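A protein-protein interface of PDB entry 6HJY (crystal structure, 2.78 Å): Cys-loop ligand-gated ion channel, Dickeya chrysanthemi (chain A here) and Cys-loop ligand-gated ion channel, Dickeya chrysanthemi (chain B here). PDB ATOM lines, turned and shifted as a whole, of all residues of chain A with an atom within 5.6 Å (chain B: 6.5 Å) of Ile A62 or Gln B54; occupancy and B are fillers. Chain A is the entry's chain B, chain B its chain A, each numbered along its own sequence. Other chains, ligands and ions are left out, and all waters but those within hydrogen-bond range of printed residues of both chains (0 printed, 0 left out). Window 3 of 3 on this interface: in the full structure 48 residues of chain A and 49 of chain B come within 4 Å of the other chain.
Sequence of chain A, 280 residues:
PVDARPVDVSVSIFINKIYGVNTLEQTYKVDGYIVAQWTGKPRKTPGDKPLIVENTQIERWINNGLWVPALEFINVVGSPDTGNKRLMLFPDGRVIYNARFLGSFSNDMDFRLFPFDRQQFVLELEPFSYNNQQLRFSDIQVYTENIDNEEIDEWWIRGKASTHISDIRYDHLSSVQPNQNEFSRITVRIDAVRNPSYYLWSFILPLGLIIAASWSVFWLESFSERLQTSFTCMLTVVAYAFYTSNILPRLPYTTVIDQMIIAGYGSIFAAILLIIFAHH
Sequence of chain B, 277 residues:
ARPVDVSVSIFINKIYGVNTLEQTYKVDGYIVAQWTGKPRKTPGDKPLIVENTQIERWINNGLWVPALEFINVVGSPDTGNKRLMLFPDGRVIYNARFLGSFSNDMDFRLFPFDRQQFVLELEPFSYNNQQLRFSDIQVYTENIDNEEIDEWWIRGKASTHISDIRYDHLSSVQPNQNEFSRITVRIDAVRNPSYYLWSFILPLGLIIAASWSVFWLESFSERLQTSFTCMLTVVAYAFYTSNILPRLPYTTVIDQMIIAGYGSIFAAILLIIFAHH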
ATOM      1  N   ILE A  58      -8.039  -1.833 -25.945  1.00  0.00           N
ATOM      2  CA  ILE A  58      -7.922  -0.891 -24.816  1.00  0.00           C
ATOM      3  C   ILE A  58      -8.574   0.440 -25.204  1.00  0.00           C
ATOM      4  O   ILE A  58      -9.371   0.982 -24.433  1.00  0.00           O
ATOM      5  CB  ILE A  58      -6.430  -0.697 -24.343  1.00  0.00           C
ATOM      6  CG1 ILE A  58      -5.900  -1.970 -23.626  1.00  0.00           C
ATOM      7  CG2 ILE A  58      -6.252   0.576 -23.453  1.00  0.00           C
ATOM      8  CD1 ILE A  58      -4.482  -1.959 -23.109  1.00  0.00           C
ATOM      9  N   GLU A  59      -8.277   0.925 -26.438  1.00  0.00           N
ATOM     10  CA  GLU A  59      -8.819   2.163 -26.995  1.00  0.00           C
ATOM     11  C   GLU A  59     -10.329   2.167 -27.056  1.00  0.00           C
ATOM     12  O   GLU A  59     -10.944   3.138 -26.602  1.00  0.00           O
ATOM     13  CB  GLU A  59      -8.231   2.520 -28.369  1.00  0.00           C
ATOM     14  CG  GLU A  59      -8.488   3.981 -28.741  1.00  0.00           C
ATOM     15  CD  GLU A  59      -8.001   5.002 -27.726  1.00  0.00           C
ATOM     16  OE1 GLU A  59      -6.824   4.905 -27.310  1.00  0.00           O
ATOM     17  OE2 GLU A  59      -8.764   5.943 -27.406  1.00  0.00           O
ATOM     18  N   ARG A  60     -10.924   1.062 -27.550  1.00  0.00           N
ATOM     19  CA  ARG A  60     -12.373   0.873 -27.656  1.00  0.00           C
ATOM     20  C   ARG A  60     -13.069   1.106 -26.302  1.00  0.00           C
ATOM     21  O   ARG A  60     -14.160   1.679 -26.272  1.00  0.00           O
ATOM     22  CB  ARG A  60     -12.717  -0.502 -28.265  1.00  0.00           C
ATOM     23  CG  ARG A  60     -12.239  -0.637 -29.714  1.00  0.00           C
ATOM     24  CD  ARG A  60     -12.680  -1.945 -30.352  1.00  0.00           C
ATOM     25  NE  ARG A  60     -14.131  -1.983 -30.555  1.00  0.00           N
ATOM     26  CZ  ARG A  60     -14.945  -2.917 -30.068  1.00  0.00           C
ATOM     27  NH1 ARG A  60     -14.461  -3.919 -29.344  1.00  0.00           N
ATOM     28  NH2 ARG A  60     -16.248  -2.866 -30.316  1.00  0.00           N
ATOM     29  N   TRP A  61     -12.403   0.718 -25.189  1.00  0.00           N
ATOM     30  CA  TRP A  61     -12.884   0.911 -23.816  1.00  0.00           C
ATOM     31  C   TRP A  61     -12.781   2.365 -23.370  1.00  0.00           C
ATOM     32  O   TRP A  61     -13.676   2.835 -22.665  1.00  0.00           O
ATOM     33  CB  TRP A  61     -12.150  -0.012 -22.840  1.00  0.00           C
ATOM     34  CG  TRP A  61     -12.690  -1.407 -22.863  1.00  0.00           C
ATOM     35  CD1 TRP A  61     -12.462  -2.354 -23.814  1.00  0.00           C
ATOM     36  CD2 TRP A  61     -13.612  -1.986 -21.932  1.00  0.00           C
ATOM     37  NE1 TRP A  61     -13.167  -3.498 -23.524  1.00  0.00           N
ATOM     38  CE2 TRP A  61     -13.884  -3.300 -22.372  1.00  0.00           C
ATOM     39  CE3 TRP A  61     -14.244  -1.516 -20.768  1.00  0.00           C
ATOM     40  CZ2 TRP A  61     -14.754  -4.155 -21.687  1.00  0.00           C
ATOM     41  CZ3 TRP A  61     -15.099  -2.366 -20.081  1.00  0.00           C
ATOM     42  CH2 TRP A  61     -15.331  -3.676 -20.528  1.00  0.00           C
ATOM     43  N   ILE A  62     -11.714   3.083 -23.802  1.00  0.00           N
ATOM     44  CA  ILE A  62     -11.479   4.500 -23.487  1.00  0.00           C
ATOM     45  C   ILE A  62     -12.538   5.357 -24.187  1.00  0.00           C
ATOM     46  O   ILE A  62     -13.154   6.207 -23.532  1.00  0.00           O
ATOM     47  CB  ILE A  62     -10.009   4.945 -23.779  1.00  0.00           C
ATOM     48  CG1 ILE A  62      -9.041   4.269 -22.789  1.00  0.00           C
ATOM     49  CG2 ILE A  62      -9.854   6.483 -23.740  1.00  0.00           C
ATOM     50  CD1 ILE A  62      -7.575   4.315 -23.151  1.00  0.00           C
ATOM     51  N   ASN A  63     -12.783   5.100 -25.498  1.00  0.00           N
ATOM     52  CA  ASN A  63     -13.813   5.801 -26.287  1.00  0.00           C
ATOM     53  C   ASN A  63     -15.189   5.645 -25.616  1.00  0.00           C
ATOM     54  O   ASN A  63     -15.964   6.602 -25.551  1.00  0.00           O
ATOM     55  CB  ASN A  63     -13.875   5.272 -27.727  1.00  0.00           C
ATOM     56  CG  ASN A  63     -12.608   5.405 -28.542  1.00  0.00           C
ATOM     57  OD1 ASN A  63     -11.716   6.202 -28.251  1.00  0.00           O
ATOM     58  ND2 ASN A  63     -12.533   4.651 -29.632  1.00  0.00           N
ATOM     59  N   ASN A  64     -15.437   4.453 -25.042  1.00  0.00           N
ATOM     60  CA  ASN A  64     -16.660   4.089 -24.340  1.00  0.00           C
ATOM     61  C   ASN A  64     -16.729   4.618 -22.896  1.00  0.00           C
ATOM     62  O   ASN A  64     -17.726   4.368 -22.214  1.00  0.00           O
ATOM     63  CB  ASN A  64     -16.900   2.585 -24.403  1.00  0.00           C
ATOM     64  CG  ASN A  64     -17.760   2.199 -25.572  1.00  0.00           C
ATOM     65  OD1 ASN A  64     -18.981   2.115 -25.456  1.00  0.00           O
ATOM     66  ND2 ASN A  64     -17.149   1.999 -26.733  1.00  0.00           N
ATOM     67  N   GLY A  65     -15.714   5.370 -22.467  1.00  0.00           N
ATOM     68  CA  GLY A  65     -15.731   6.021 -21.157  1.00  0.00           C
ATOM     69  C   GLY A  65     -14.848   5.486 -20.050  1.00  0.00           C
ATOM     70  O   GLY A  65     -14.940   5.982 -18.929  1.00  0.00           O
ATOM     71  N   LEU A  66     -13.996   4.485 -20.330  1.00  0.00           N
ATOM     72  CA  LEU A  66     -13.103   3.955 -19.295  1.00  0.00           C
ATOM     73  C   LEU A  66     -11.958   4.930 -19.039  1.00  0.00           C
ATOM     74  O   LEU A  66     -11.371   5.467 -19.983  1.00  0.00           O
ATOM     75  CB  LEU A  66     -12.589   2.544 -19.643  1.00  0.00           C
ATOM     76  CG  LEU A  66     -11.671   1.855 -18.622  1.00  0.00           C
ATOM     77  CD1 LEU A  66     -12.449   1.306 -17.432  1.00  0.00           C
ATOM     78  CD2 LEU A  66     -10.909   0.736 -19.271  1.00  0.00           C
ATOM     79  N   VAL A  68      -8.390   5.749 -18.189  1.00  0.00           N
ATOM     80  CA  VAL A  68      -7.021   5.219 -18.243  1.00  0.00           C
ATOM     81  C   VAL A  68      -6.087   6.452 -18.305  1.00  0.00           C
ATOM     82  O   VAL A  68      -5.876   7.011 -19.391  1.00  0.00           O
ATOM     83  CB  VAL A  68      -6.757   4.193 -19.392  1.00  0.00           C
ATOM     84  CG1 VAL A  68      -5.379   3.559 -19.241  1.00  0.00           C
ATOM     85  CG2 VAL A  68      -7.830   3.104 -19.441  1.00  0.00           C
ATOM     86  N   VAL B  50      -9.070  15.959 -21.639  1.00  0.00           N
ATOM     87  CA  VAL B  50      -9.178  15.118 -22.841  1.00  0.00           C
ATOM     88  C   VAL B  50      -7.724  14.770 -23.269  1.00  0.00           C
ATOM     89  O   VAL B  50      -6.907  15.671 -23.478  1.00  0.00           O
ATOM     90  CB  VAL B  50     -10.007  15.823 -23.963  1.00  0.00           C
ATOM     91  CG1 VAL B  50     -10.082  14.973 -25.217  1.00  0.00           C
ATOM     92  CG2 VAL B  50     -11.418  16.148 -23.486  1.00  0.00           C
ATOM     93  N   GLU B  51      -7.373  13.470 -23.296  1.00  0.00           N
ATOM     94  CA  GLU B  51      -6.012  13.066 -23.628  1.00  0.00           C
ATOM     95  C   GLU B  51      -5.856  12.292 -24.921  1.00  0.00           C
ATOM     96  O   GLU B  51      -6.750  11.577 -25.366  1.00  0.00           O
ATOM     97  CB  GLU B  51      -5.420  12.206 -22.507  1.00  0.00           C
ATOM     98  CG  GLU B  51      -5.112  12.909 -21.204  1.00  0.00           C
ATOM     99  CD  GLU B  51      -4.659  11.984 -20.097  1.00  0.00           C
ATOM    100  OE1 GLU B  51      -4.808  10.755 -20.243  1.00  0.00           O
ATOM    101  OE2 GLU B  51      -4.169  12.488 -19.069  1.00  0.00           O
ATOM    102  N   ASN B  52      -4.661  12.436 -25.491  1.00  0.00           N
ATOM    103  CA  ASN B  52      -4.051  11.822 -26.658  1.00  0.00           C
ATOM    104  C   ASN B  52      -5.013  11.536 -27.834  1.00  0.00           C
ATOM    105  O   ASN B  52      -5.248  12.445 -28.629  1.00  0.00           O
ATOM    106  CB  ASN B  52      -3.298  10.544 -26.251  1.00  0.00           C
ATOM    107  CG  ASN B  52      -2.069  10.831 -25.404  1.00  0.00           C
ATOM    108  OD1 ASN B  52      -1.397  11.834 -25.585  1.00  0.00           O
ATOM    109  ND2 ASN B  52      -1.752   9.961 -24.458  1.00  0.00           N
ATOM    110  N   THR B  53      -5.542  10.314 -27.941  1.00  0.00           N
ATOM    111  CA  THR B  53      -6.429   9.855 -29.018  1.00  0.00           C
ATOM    112  C   THR B  53      -7.870  10.383 -28.891  1.00  0.00           C
ATOM    113  O   THR B  53      -8.585  10.400 -29.894  1.00  0.00           O
ATOM    114  CB  THR B  53      -6.386   8.313 -29.103  1.00  0.00           C
ATOM    115  OG1 THR B  53      -6.789   7.769 -27.855  1.00  0.00           O
ATOM    116  CG2 THR B  53      -5.007   7.757 -29.506  1.00  0.00           C
ATOM    117  N   GLN B  54      -8.280  10.836 -27.679  1.00  0.00           N
ATOM    118  CA  GLN B  54      -9.612  11.378 -27.401  1.00  0.00           C
ATOM    119  C   GLN B  54      -9.793  12.765 -27.986  1.00  0.00           C
ATOM    120  O   GLN B  54     -10.923  13.138 -28.302  1.00  0.00           O
ATOM    121  CB  GLN B  54      -9.939  11.352 -25.897  1.00  0.00           C
ATOM    122  CG  GLN B  54     -10.074   9.946 -25.306  1.00  0.00           C
ATOM    123  CD  GLN B  54     -10.953   9.081 -26.163  1.00  0.00           C
ATOM    124  OE1 GLN B  54     -12.158   9.296 -26.259  1.00  0.00           O
ATOM    125  NE2 GLN B  54     -10.341   8.187 -26.910  1.00  0.00           N
ATOM    126  N   ILE B  55      -8.669  13.518 -28.159  1.00  0.00           N
ATOM    127  CA  ILE B  55      -8.602  14.863 -28.756  1.00  0.00           C
ATOM    128  C   ILE B  55      -9.233  14.809 -30.141  1.00  0.00           C
ATOM    129  O   ILE B  55     -10.108  15.616 -30.452  1.00  0.00           O
ATOM    130  CB  ILE B  55      -7.134  15.403 -28.789  1.00  0.00           C
ATOM    131  CG1 ILE B  55      -6.630  15.673 -27.353  1.00  0.00           C
ATOM    132  CG2 ILE B  55      -6.982  16.659 -29.689  1.00  0.00           C
ATOM    133  CD1 ILE B  55      -5.180  15.919 -27.194  1.00  0.00           C
ATOM    134  N   GLU B  56      -8.850  13.788 -30.922  1.00  0.00           N
ATOM    135  CA  GLU B  56      -9.346  13.517 -32.259  1.00  0.00           C
ATOM    136  C   GLU B  56     -10.866  13.357 -32.312  1.00  0.00           C
ATOM    137  O   GLU B  56     -11.497  13.871 -33.238  1.00  0.00           O
ATOM    138  CB  GLU B  56      -8.620  12.304 -32.869  1.00  0.00           C
ATOM    139  CG  GLU B  56      -8.530  12.334 -34.389  1.00  0.00           C
ATOM    140  CD  GLU B  56      -8.442  13.729 -34.986  1.00  0.00           C
ATOM    141  OE1 GLU B  56      -7.381  14.375 -34.825  1.00  0.00           O
ATOM    142  OE2 GLU B  56      -9.432  14.184 -35.601  1.00  0.00           O
ATOM    143  N   ARG B  57     -11.449  12.722 -31.277  1.00  0.00           N
ATOM    144  CA  ARG B  57     -12.895  12.513 -31.150  1.00  0.00           C
ATOM    145  C   ARG B  57     -13.626  13.840 -30.924  1.00  0.00           C
ATOM    146  O   ARG B  57     -14.726  14.035 -31.450  1.00  0.00           O
ATOM    147  CB  ARG B  57     -13.222  11.477 -30.059  1.00  0.00           C
ATOM    148  CG  ARG B  57     -12.712  10.079 -30.416  1.00  0.00           C
ATOM    149  CD  ARG B  57     -13.140   9.008 -29.420  1.00  0.00           C
ATOM    150  NE  ARG B  57     -14.593   8.819 -29.412  1.00  0.00           N
ATOM    151  CZ  ARG B  57     -15.370   8.955 -28.340  1.00  0.00           C
ATOM    152  NH1 ARG B  57     -14.844   9.275 -27.164  1.00  0.00           N
ATOM    153  NH2 ARG B  57     -16.680   8.759 -28.433  1.00  0.00           N
ATOM    154  N   TRP B  58     -12.988  14.770 -30.192  1.00  0.00           N
ATOM    155  CA  TRP B  58     -13.534  16.099 -29.932  1.00  0.00           C
ATOM    156  C   TRP B  58     -13.470  16.991 -31.157  1.00  0.00           C
ATOM    157  O   TRP B  58     -14.401  17.765 -31.378  1.00  0.00           O
ATOM    158  CB  TRP B  58     -12.829  16.748 -28.744  1.00  0.00           C
ATOM    159  CG  TRP B  58     -13.404  16.279 -27.449  1.00  0.00           C
ATOM    160  CD1 TRP B  58     -13.172  15.085 -26.833  1.00  0.00           C
ATOM    161  CD2 TRP B  58     -14.414  16.939 -26.681  1.00  0.00           C
ATOM    162  NE1 TRP B  58     -13.931  14.986 -25.689  1.00  0.00           N
ATOM    163  CE2 TRP B  58     -14.706  16.111 -25.573  1.00  0.00           C
ATOM    164  CE3 TRP B  58     -15.090  18.163 -26.811  1.00  0.00           C
ATOM    165  CZ2 TRP B  58     -15.654  16.463 -24.610  1.00  0.00           C
ATOM    166  CZ3 TRP B  58     -16.003  18.527 -25.837  1.00  0.00           C
ATOM    167  CH2 TRP B  58     -16.268  17.690 -24.743  1.00  0.00           C
ATOM    168  N   ILE B  59     -12.396  16.864 -31.967  1.00  0.00           N
ATOM    169  CA  ILE B  59     -12.200  17.645 -33.190  1.00  0.00           C
ATOM    170  C   ILE B  59     -13.253  17.249 -34.228  1.00  0.00           C
ATOM    171  O   ILE B  59     -13.910  18.134 -34.782  1.00  0.00           O
ATOM    172  CB  ILE B  59     -10.732  17.596 -33.709  1.00  0.00           C
ATOM    173  CG1 ILE B  59      -9.783  18.268 -32.698  1.00  0.00           C
ATOM    174  CG2 ILE B  59     -10.606  18.295 -35.066  1.00  0.00           C
ATOM    175  CD1 ILE B  59      -8.298  18.038 -32.934  1.00  0.00           C
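The side-chain carboxylate (OE2) of Glu A59 sits at hydrogen-bond distance from the side-chain hydroxyl (OG1) of Thr B53 (2.7 Å).
NE2 of Gln B54 lies within hydrogen-bond range of OE2 of Glu A59, at 2.8 Å.
NE2 of Gln B54 lies within hydrogen-bond range of OD1 of Asn A63 (2.8 Å).
The guanidinium group of Arg B57 sits at hydrogen-bond distance from the backbone carbonyl oxygen of Asn A63 (3.3 Å).
NH1 of Arg B57 sits at hydrogen-bond distance from OE1 of Gln B54, 2.8 Å away.
The side-chain amide oxygen (OD1) of Asn A63 sits close to the side-chain carboxylate (OE2) of Glu A59.
Among the printed residues, merely in contact across the chains: Ile A62 with Gln B54 and Val A68 with Glu B51.
Of chain B, only Gln B54 comes within 4 Å of Ile A62.
Gln B54 touches just these residues of chain A: Glu A59 (2.8 Å), Ile A62 (3.6 Å) and Asn A63 (2.8 Å).
Printed residues of chain A within 4 Å of Thr B53: Glu A59 (2.7 Å).
Of the printed residues of chain A, Glu B51 touches Val A68 (3.99 Å).
Printed residues of chain A within 4 Å of Arg B57: Asn A63 (3.3 Å).
Printed residues of chain B within 4 Å of Glu A59: Thr B53 and Gln B54.
Of the printed residues of chain B, Asn A63 touches Gln B54 and Arg B57.
Of the 10 printed residues of chain A, 4 touch a printed residue of chain B.
Hydrophobic or aromatic side chains of chain A that line the printed part of chain B: Ile A62.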
